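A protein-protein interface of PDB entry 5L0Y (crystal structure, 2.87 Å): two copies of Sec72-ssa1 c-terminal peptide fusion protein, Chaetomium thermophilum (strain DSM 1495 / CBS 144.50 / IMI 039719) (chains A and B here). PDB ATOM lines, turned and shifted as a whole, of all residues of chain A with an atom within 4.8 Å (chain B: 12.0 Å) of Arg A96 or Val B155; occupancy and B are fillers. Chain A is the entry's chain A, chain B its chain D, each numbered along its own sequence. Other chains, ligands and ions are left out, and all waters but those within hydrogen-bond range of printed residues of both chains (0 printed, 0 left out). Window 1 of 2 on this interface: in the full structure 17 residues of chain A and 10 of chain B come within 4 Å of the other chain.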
ATOM      1  N   SER A  60      17.240 -17.753  -2.885  1.00  0.00           N
ATOM      2  CA  SER A  60      15.797 -17.561  -2.932  1.00  0.00           C
ATOM      3  C   SER A  60      15.204 -18.217  -4.186  1.00  0.00           C
ATOM      4  O   SER A  60      14.190 -18.926  -4.109  1.00  0.00           O
ATOM      5  CB  SER A  60      15.459 -16.073  -2.883  1.00  0.00           C
ATOM      6  OG  SER A  60      14.064 -15.876  -2.738  1.00  0.00           O
ATOM      7  N   ASN A  61      15.859 -18.005  -5.326  1.00  0.00           N
ATOM      8  CA  ASN A  61      15.422 -18.588  -6.597  1.00  0.00           C
ATOM      9  C   ASN A  61      15.401 -20.109  -6.586  1.00  0.00           C
ATOM     10  O   ASN A  61      14.412 -20.731  -6.992  1.00  0.00           O
ATOM     11  CB  ASN A  61      16.317 -18.111  -7.742  1.00  0.00           C
ATOM     12  CG  ASN A  61      15.915 -16.748  -8.267  1.00  0.00           C
ATOM     13  OD1 ASN A  61      15.022 -16.096  -7.721  1.00  0.00           O
ATOM     14  ND2 ASN A  61      16.573 -16.310  -9.336  1.00  0.00           N
ATOM     15  N   ALA A  63      15.231 -21.966  -4.040  1.00  0.00           N
ATOM     16  CA  ALA A  63      14.167 -22.365  -3.120  1.00  0.00           C
ATOM     17  C   ALA A  63      12.826 -22.402  -3.841  1.00  0.00           C
ATOM     18  O   ALA A  63      12.076 -23.373  -3.717  1.00  0.00           O
ATOM     19  CB  ALA A  63      14.101 -21.432  -1.934  1.00  0.00           C
ATOM     20  N   GLN A  64      12.527 -21.351  -4.601  1.00  0.00           N
ATOM     21  CA  GLN A  64      11.288 -21.321  -5.375  1.00  0.00           C
ATOM     22  C   GLN A  64      11.190 -22.516  -6.329  1.00  0.00           C
ATOM     23  O   GLN A  64      10.175 -23.236  -6.343  1.00  0.00           O
ATOM     24  CB  GLN A  64      11.174 -20.012  -6.152  1.00  0.00           C
ATOM     25  CG  GLN A  64       9.887 -19.886  -6.937  1.00  0.00           C
ATOM     26  CD  GLN A  64       8.656 -19.946  -6.051  1.00  0.00           C
ATOM     27  OE1 GLN A  64       8.653 -19.414  -4.938  1.00  0.00           O
ATOM     28  NE2 GLN A  64       7.605 -20.598  -6.539  1.00  0.00           N
ATOM     29  N   MET A  67      10.281 -25.513  -4.558  1.00  0.00           N
ATOM     30  CA  MET A  67       8.883 -25.541  -4.143  1.00  0.00           C
ATOM     31  C   MET A  67       7.988 -25.947  -5.315  1.00  0.00           C
ATOM     32  O   MET A  67       6.906 -26.521  -5.126  1.00  0.00           O
ATOM     33  CB  MET A  67       8.456 -24.184  -3.580  1.00  0.00           C
ATOM     34  CG  MET A  67       9.229 -23.760  -2.346  1.00  0.00           C
ATOM     35  SD  MET A  67       8.818 -22.094  -1.817  1.00  0.00           S
ATOM     36  CE  MET A  67       7.121 -22.338  -1.273  1.00  0.00           C
ATOM     37  N   ALA A  79      15.963 -20.982   1.374  1.00  0.00           N
ATOM     38  CA  ALA A  79      15.348 -19.721   1.752  1.00  0.00           C
ATOM     39  C   ALA A  79      15.977 -19.200   3.039  1.00  0.00           C
ATOM     40  O   ALA A  79      16.180 -17.995   3.197  1.00  0.00           O
ATOM     41  CB  ALA A  79      13.857 -19.891   1.913  1.00  0.00           C
ATOM     42  N   LYS A  92      10.480 -12.256  -0.260  1.00  0.00           N
ATOM     43  CA  LYS A  92      10.229 -13.535  -0.902  1.00  0.00           C
ATOM     44  C   LYS A  92      10.907 -14.708  -0.197  1.00  0.00           C
ATOM     45  O   LYS A  92      10.362 -15.799  -0.167  1.00  0.00           O
ATOM     46  CB  LYS A  92      10.678 -13.488  -2.356  1.00  0.00           C
ATOM     47  CG  LYS A  92       9.635 -12.937  -3.299  1.00  0.00           C
ATOM     48  CD  LYS A  92      10.248 -12.611  -4.650  1.00  0.00           C
ATOM     49  CE  LYS A  92       9.177 -12.444  -5.706  1.00  0.00           C
ATOM     50  NZ  LYS A  92       9.706 -11.813  -6.945  1.00  0.00           N
ATOM     51  N   ALA A  93      12.094 -14.492   0.360  1.00  0.00           N
ATOM     52  CA  ALA A  93      12.802 -15.578   1.035  1.00  0.00           C
ATOM     53  C   ALA A  93      12.076 -15.969   2.319  1.00  0.00           C
ATOM     54  O   ALA A  93      11.729 -17.147   2.517  1.00  0.00           O
ATOM     55  CB  ALA A  93      14.236 -15.181   1.325  1.00  0.00           C
ATOM     56  N   TRP A  94      11.853 -14.975   3.182  1.00  0.00           N
ATOM     57  CA  TRP A  94      11.043 -15.140   4.392  1.00  0.00           C
ATOM     58  C   TRP A  94       9.763 -15.889   4.074  1.00  0.00           C
ATOM     59  O   TRP A  94       9.411 -16.874   4.729  1.00  0.00           O
ATOM     60  CB  TRP A  94      10.680 -13.788   5.015  1.00  0.00           C
ATOM     61  CG  TRP A  94      11.825 -13.025   5.605  1.00  0.00           C
ATOM     62  CD1 TRP A  94      12.508 -11.990   5.028  1.00  0.00           C
ATOM     63  CD2 TRP A  94      12.413 -13.219   6.897  1.00  0.00           C
ATOM     64  NE1 TRP A  94      13.485 -11.536   5.878  1.00  0.00           N
ATOM     65  CE2 TRP A  94      13.448 -12.275   7.032  1.00  0.00           C
ATOM     66  CE3 TRP A  94      12.172 -14.108   7.948  1.00  0.00           C
ATOM     67  CZ2 TRP A  94      14.233 -12.189   8.176  1.00  0.00           C
ATOM     68  CZ3 TRP A  94      12.950 -14.018   9.085  1.00  0.00           C
ATOM     69  CH2 TRP A  94      13.970 -13.071   9.188  1.00  0.00           C
ATOM     70  N   TYR A  95       9.075 -15.405   3.049  1.00  0.00           N
ATOM     71  CA  TYR A  95       7.817 -15.988   2.642  1.00  0.00           C
ATOM     72  C   TYR A  95       7.979 -17.451   2.288  1.00  0.00           C
ATOM     73  O   TYR A  95       7.247 -18.312   2.795  1.00  0.00           O
ATOM     74  CB  TYR A  95       7.236 -15.241   1.448  1.00  0.00           C
ATOM     75  CG  TYR A  95       5.881 -15.760   1.037  1.00  0.00           C
ATOM     76  CD1 TYR A  95       4.718 -15.177   1.517  1.00  0.00           C
ATOM     77  CD2 TYR A  95       5.763 -16.845   0.184  1.00  0.00           C
ATOM     78  CE1 TYR A  95       3.476 -15.655   1.149  1.00  0.00           C
ATOM     79  CE2 TYR A  95       4.530 -17.333  -0.184  1.00  0.00           C
ATOM     80  CZ  TYR A  95       3.393 -16.731   0.293  1.00  0.00           C
ATOM     81  OH  TYR A  95       2.177 -17.235  -0.095  1.00  0.00           O
ATOM     82  N   ARG A  96       8.928 -17.716   1.397  1.00  0.00           N
ATOM     83  CA  ARG A  96       9.126 -19.046   0.849  1.00  0.00           C
ATOM     84  C   ARG A  96       9.376 -20.050   1.952  1.00  0.00           C
ATOM     85  O   ARG A  96       8.747 -21.114   1.974  1.00  0.00           O
ATOM     86  CB  ARG A  96      10.278 -19.034  -0.162  1.00  0.00           C
ATOM     87  CG  ARG A  96       9.827 -18.647  -1.562  1.00  0.00           C
ATOM     88  CD  ARG A  96      10.927 -18.051  -2.427  1.00  0.00           C
ATOM     89  NE  ARG A  96      10.343 -17.433  -3.616  1.00  0.00           N
ATOM     90  CZ  ARG A  96      11.004 -16.678  -4.487  1.00  0.00           C
ATOM     91  NH1 ARG A  96      12.297 -16.434  -4.323  1.00  0.00           N
ATOM     92  NH2 ARG A  96      10.366 -16.167  -5.532  1.00  0.00           N
ATOM     93  N   ARG A  97      10.262 -19.705   2.883  1.00  0.00           N
ATOM     94  CA  ARG A  97      10.502 -20.606   4.001  1.00  0.00           C
ATOM     95  C   ARG A  97       9.248 -20.755   4.853  1.00  0.00           C
ATOM     96  O   ARG A  97       8.965 -21.849   5.348  1.00  0.00           O
ATOM     97  CB  ARG A  97      11.667 -20.132   4.865  1.00  0.00           C
ATOM     98  CG  ARG A  97      11.913 -21.036   6.059  1.00  0.00           C
ATOM     99  CD  ARG A  97      13.305 -20.848   6.643  1.00  0.00           C
ATOM    100  NE  ARG A  97      13.399 -21.372   8.003  1.00  0.00           N
ATOM    101  CZ  ARG A  97      13.658 -22.643   8.300  1.00  0.00           C
ATOM    102  NH1 ARG A  97      13.854 -23.530   7.329  1.00  0.00           N
ATOM    103  NH2 ARG A  97      13.724 -23.028   9.567  1.00  0.00           N
ATOM    104  N   GLY A  98       8.500 -19.664   5.023  1.00  0.00           N
ATOM    105  CA  GLY A  98       7.247 -19.717   5.761  1.00  0.00           C
ATOM    106  C   GLY A  98       6.310 -20.784   5.217  1.00  0.00           C
ATOM    107  O   GLY A  98       5.843 -21.664   5.963  1.00  0.00           O
ATOM    108  N   LYS A  99       6.053 -20.728   3.911  1.00  0.00           N
ATOM    109  CA  LYS A  99       5.204 -21.729   3.266  1.00  0.00           C
ATOM    110  C   LYS A  99       5.812 -23.123   3.328  1.00  0.00           C
ATOM    111  O   LYS A  99       5.087 -24.110   3.426  1.00  0.00           O
ATOM    112  CB  LYS A  99       4.928 -21.360   1.804  1.00  0.00           C
ATOM    113  CG  LYS A  99       3.473 -21.043   1.489  1.00  0.00           C
ATOM    114  CD  LYS A  99       3.106 -21.487   0.078  1.00  0.00           C
ATOM    115  CE  LYS A  99       2.635 -22.940   0.056  1.00  0.00           C
ATOM    116  NZ  LYS A  99       2.765 -23.578  -1.290  1.00  0.00           N
ATOM    117  N   CYS A 100       7.137 -23.210   3.249  1.00  0.00           N
ATOM    118  CA  CYS A 100       7.786 -24.514   3.303  1.00  0.00           C
ATOM    119  C   CYS A 100       7.570 -25.176   4.659  1.00  0.00           C
ATOM    120  O   CYS A 100       7.327 -26.376   4.743  1.00  0.00           O
ATOM    121  CB  CYS A 100       9.279 -24.390   3.010  1.00  0.00           C
ATOM    122  SG  CYS A 100       9.652 -24.063   1.286  1.00  0.00           S
ATOM    123  N   GLU A 126       2.706  -9.200   1.829  1.00  0.00           N
ATOM    124  CA  GLU A 126       2.614 -10.623   1.464  1.00  0.00           C
ATOM    125  C   GLU A 126       2.982 -11.571   2.600  1.00  0.00           C
ATOM    126  O   GLU A 126       2.273 -12.558   2.871  1.00  0.00           O
ATOM    127  CB  GLU A 126       3.486 -10.922   0.256  1.00  0.00           C
ATOM    128  CG  GLU A 126       2.797 -11.831  -0.739  1.00  0.00           C
ATOM    129  CD  GLU A 126       2.654 -11.184  -2.098  1.00  0.00           C
ATOM    130  OE1 GLU A 126       3.684 -11.009  -2.780  1.00  0.00           O
ATOM    131  OE2 GLU A 126       1.517 -10.841  -2.487  1.00  0.00           O
ATOM    132  N   LYS B 142     -10.093 -11.110   1.620  1.00  0.00           N
ATOM    133  CA  LYS B 142      -8.859 -11.369   0.880  1.00  0.00           C
ATOM    134  C   LYS B 142      -9.124 -11.907  -0.529  1.00  0.00           C
ATOM    135  O   LYS B 142      -8.516 -11.454  -1.531  1.00  0.00           O
ATOM    136  CB  LYS B 142      -7.970 -12.342   1.643  1.00  0.00           C
ATOM    137  CG  LYS B 142      -6.531 -12.273   1.181  1.00  0.00           C
ATOM    138  CD  LYS B 142      -6.072 -10.814   1.094  1.00  0.00           C
ATOM    139  CE  LYS B 142      -5.822 -10.201   2.478  1.00  0.00           C
ATOM    140  NZ  LYS B 142      -5.991  -8.712   2.498  1.00  0.00           N
ATOM    141  N   ASP B 146      -8.162 -10.254  -4.331  1.00  0.00           N
ATOM    142  CA  ASP B 146      -7.370 -10.840  -5.403  1.00  0.00           C
ATOM    143  C   ASP B 146      -8.067 -10.730  -6.758  1.00  0.00           C
ATOM    144  O   ASP B 146      -7.471 -10.370  -7.761  1.00  0.00           O
ATOM    145  CB  ASP B 146      -6.905 -12.267  -5.040  1.00  0.00           C
ATOM    146  CG  ASP B 146      -7.622 -13.354  -5.802  1.00  0.00           C
ATOM    147  OD1 ASP B 146      -7.540 -13.360  -7.041  1.00  0.00           O
ATOM    148  OD2 ASP B 146      -8.259 -14.197  -5.156  1.00  0.00           O
ATOM    149  N   ASN B 150      -6.969  -9.080 -10.333  1.00  0.00           N
ATOM    150  CA  ASN B 150      -6.442 -10.318 -10.873  1.00  0.00           C
ATOM    151  C   ASN B 150      -5.177 -10.744 -10.170  1.00  0.00           C
ATOM    152  O   ASN B 150      -4.803 -10.151  -9.175  1.00  0.00           O
ATOM    153  CB  ASN B 150      -6.188 -10.174 -12.363  1.00  0.00           C
ATOM    154  CG  ASN B 150      -6.485 -11.436 -13.113  1.00  0.00           C
ATOM    155  OD1 ASN B 150      -7.500 -12.078 -12.881  1.00  0.00           O
ATOM    156  ND2 ASN B 150      -5.598 -11.803 -14.015  1.00  0.00           N
ATOM    157  N   PRO B 153       0.499 -12.179  -8.133  1.00  0.00           N
ATOM    158  CA  PRO B 153       1.083 -13.519  -8.058  1.00  0.00           C
ATOM    159  C   PRO B 153       2.600 -13.433  -8.013  1.00  0.00           C
ATOM    160  O   PRO B 153       3.282 -14.364  -8.441  1.00  0.00           O
ATOM    161  CB  PRO B 153       0.604 -14.174  -9.350  1.00  0.00           C
ATOM    162  CG  PRO B 153       0.556 -13.031 -10.323  1.00  0.00           C
ATOM    163  CD  PRO B 153       0.257 -11.769  -9.526  1.00  0.00           C
ATOM    164  N   THR B 154       3.100 -12.311  -7.499  1.00  0.00           N
ATOM    165  CA  THR B 154       4.521 -11.992  -7.513  1.00  0.00           C
ATOM    166  C   THR B 154       5.382 -13.035  -6.800  1.00  0.00           C
ATOM    167  O   THR B 154       6.550 -13.212  -7.142  1.00  0.00           O
ATOM    168  CB  THR B 154       4.791 -10.613  -6.867  1.00  0.00           C
ATOM    169  OG1 THR B 154       4.598 -10.692  -5.449  1.00  0.00           O
ATOM    170  CG2 THR B 154       3.859  -9.556  -7.444  1.00  0.00           C
ATOM    171  N   VAL B 155       4.801 -13.726  -5.825  1.00  0.00           N
ATOM    172  CA  VAL B 155       5.539 -14.682  -5.002  1.00  0.00           C
ATOM    173  C   VAL B 155       6.204 -15.804  -5.797  1.00  0.00           C
ATOM    174  O   VAL B 155       7.343 -16.187  -5.520  1.00  0.00           O
ATOM    175  CB  VAL B 155       4.623 -15.327  -3.963  1.00  0.00           C
ATOM    176  CG1 VAL B 155       5.413 -16.309  -3.129  1.00  0.00           C
ATOM    177  CG2 VAL B 155       3.968 -14.263  -3.102  1.00  0.00           C
ATOM    178  N   GLU B 156       5.478 -16.336  -6.773  1.00  0.00           N
ATOM    179  CA  GLU B 156       5.992 -17.412  -7.605  1.00  0.00           C
ATOM    180  C   GLU B 156       7.099 -16.910  -8.519  1.00  0.00           C
ATOM    181  O   GLU B 156       8.055 -17.633  -8.813  1.00  0.00           O
ATOM    182  CB  GLU B 156       4.866 -18.029  -8.442  1.00  0.00           C
ATOM    183  CG  GLU B 156       3.633 -18.457  -7.653  1.00  0.00           C
ATOM    184  CD  GLU B 156       3.823 -19.778  -6.933  1.00  0.00           C
ATOM    185  OE1 GLU B 156       2.815 -20.472  -6.679  1.00  0.00           O
ATOM    186  OE2 GLU B 156       4.979 -20.123  -6.617  1.00  0.00           O
ATOM    187  N   GLU B 157       6.958 -15.666  -8.966  1.00  0.00           N
ATOM    188  CA  GLU B 157       7.900 -15.086  -9.910  1.00  0.00           C
ATOM    189  C   GLU B 157       9.320 -15.114  -9.371  1.00  0.00           C
ATOM    190  O   GLU B 157       9.557 -15.036  -8.164  1.00  0.00           O
ATOM    191  CB  GLU B 157       7.497 -13.652 -10.251  1.00  0.00           C
ATOM    192  CG  GLU B 157       6.000 -13.433 -10.255  1.00  0.00           C
ATOM    193  CD  GLU B 157       5.467 -12.968 -11.590  1.00  0.00           C
ATOM    194  OE1 GLU B 157       5.603 -11.766 -11.903  1.00  0.00           O
ATOM    195  OE2 GLU B 157       4.896 -13.810 -12.315  1.00  0.00           O
ATOM    196  N   VAL B 158      10.265 -15.237 -10.289  1.00  0.00           N
ATOM    197  CA  VAL B 158      11.651 -15.415  -9.918  1.00  0.00           C
ATOM    198  C   VAL B 158      12.461 -14.240 -10.462  1.00  0.00           C
ATOM    199  O   VAL B 158      12.277 -13.824 -11.609  1.00  0.00           O
ATOM    200  CB  VAL B 158      12.164 -16.775 -10.438  1.00  0.00           C
ATOM    201  CG1 VAL B 158      13.347 -16.615 -11.339  1.00  0.00           C
ATOM    202  CG2 VAL B 158      12.483 -17.700  -9.282  1.00  0.00           C
ATOM    203  N   ASP B 159      13.323 -13.671  -9.629  1.00  0.00           N
ATOM    204  CA  ASP B 159      14.164 -12.570 -10.082  1.00  0.00           C
ATOM    205  C   ASP B 159      15.591 -13.045 -10.256  1.00  0.00           C
ATOM    206  O   ASP B 159      16.458 -12.267 -10.638  1.00  0.00           O
ATOM    207  CB  ASP B 159      14.120 -11.387  -9.112  1.00  0.00           C
ATOM    208  CG  ASP B 159      13.212 -11.629  -7.932  1.00  0.00           C
ATOM    209  OD1 ASP B 159      13.193 -12.762  -7.404  1.00  0.00           O
ATOM    210  OD2 ASP B 159      12.513 -10.676  -7.530  1.00  0.00           O
ATOM    211  OXT ASP B 159      15.917 -14.208 -10.022  1.00  0.00           O
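Among the printed residues, merely in contact across the chains: Tyr A95 with Val B155 (3.2 Å), Glu A126 with Val B155 (3.3 Å), Asn A61 with Val B158 (3.4 Å) and Gln A64 with Val B155 (3.5 Å).
Printed residues of chain B within 4 Å of Asn A61: Val B158 (3.4 Å) and Asp B159 (2.3 Å).
Ala A63 touches none of the printed residues of chain B.
No residue of chain B comes within 4 Å of Ala A79.
No residue of chain B comes within 4 Å of Ala A93.
Tyr A95 touches just one residue of chain B: Val B155 (3.2 Å).
Of chain B, only Val B155 and Glu B157 come within 4 Å of Arg A96.
No residue of chain B comes within 4 Å of Lys A99.
Cys A100 touches none of the printed residues of chain B.
Of the printed residues of chain A, Thr B154 touches Lys A92 (3.1 Å) and Glu A126 (2.8 Å).
Val B155 touches just these residues of chain A: Gln A64, Tyr A95, Arg A96 and Glu A126.
Printed residues of chain A within 4 Å of Glu B156: Gln A64 (2.7 Å).
Of the printed residues of chain A, Glu B157 touches Lys A92 and Arg A96.
Of the printed residues of chain A, Val B158 touches Asn A61 (3.4 Å).
Printed residues of chain A within 4 Å of Asp B159: Asn A61 (2.3 Å) and Lys A92 (3.1 Å).
The nearest residue of chain A that does not touch Val B155 is Lys A92 (4.2 Å).
OG of Ser A60 is in hydrogen-bond range of NH1 of Arg A96, at 2.4 Å.
OE1 of Gln A64 is in hydrogen-bond range of NE of Arg A96, at 2.9 Å.
The backbone carbonyl oxygen (O) of Arg A96 sits at hydrogen-bond distance from the side-chain sulfur (SG) of Cys A100 (3.2 Å).
OD1 of Asn A61 lies close to OXT of Asp B159, 3.1 Å away.
The side-chain carboxylate of Glu B156 sits at hydrogen-bond distance from the side-chain amide nitrogen of Gln A64.
The side-chain amino group (NZ) of Lys A92 sits close to the backbone carbonyl oxygen (O) of Thr B154, at 3.5 Å.
NZ of Lys A92 is in hydrogen-bond range of O of Glu B157, at 3.4 Å.
The side-chain amino group of Lys A92 is in salt-bridge range of the side-chain carboxylate of Asp B159 (3.1 Å).
O of Val B155 sits at hydrogen-bond distance from NH2 of Arg A96 (3.0 Å).
The backbone carbonyl oxygen (O) of Glu B157 sits at hydrogen-bond distance from the guanidinium group (NH2) of Arg A96, at 3.0 Å.
The side-chain hydroxyl (OG1) of Thr B154 is in hydrogen-bond range of the side-chain carboxylate (OE1) of Glu A126, at 2.8 Å.
Printed residues of chain A that touch a printed residue of chain B: Asn A61, Gln A64, Lys A92, Tyr A95, Arg A96 and Glu A126.
Among the printed residues, Asp or Glu carboxylates within 4 Å of a Lys or Arg side-chain nitrogen of the other chain: Lys A92 with Asp B159 (3.1 Å).
No position is printed for both chains.
Of the 12 pairs that touch across the chains among the printed residues, none has its exchanged pair printed and touching as well.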
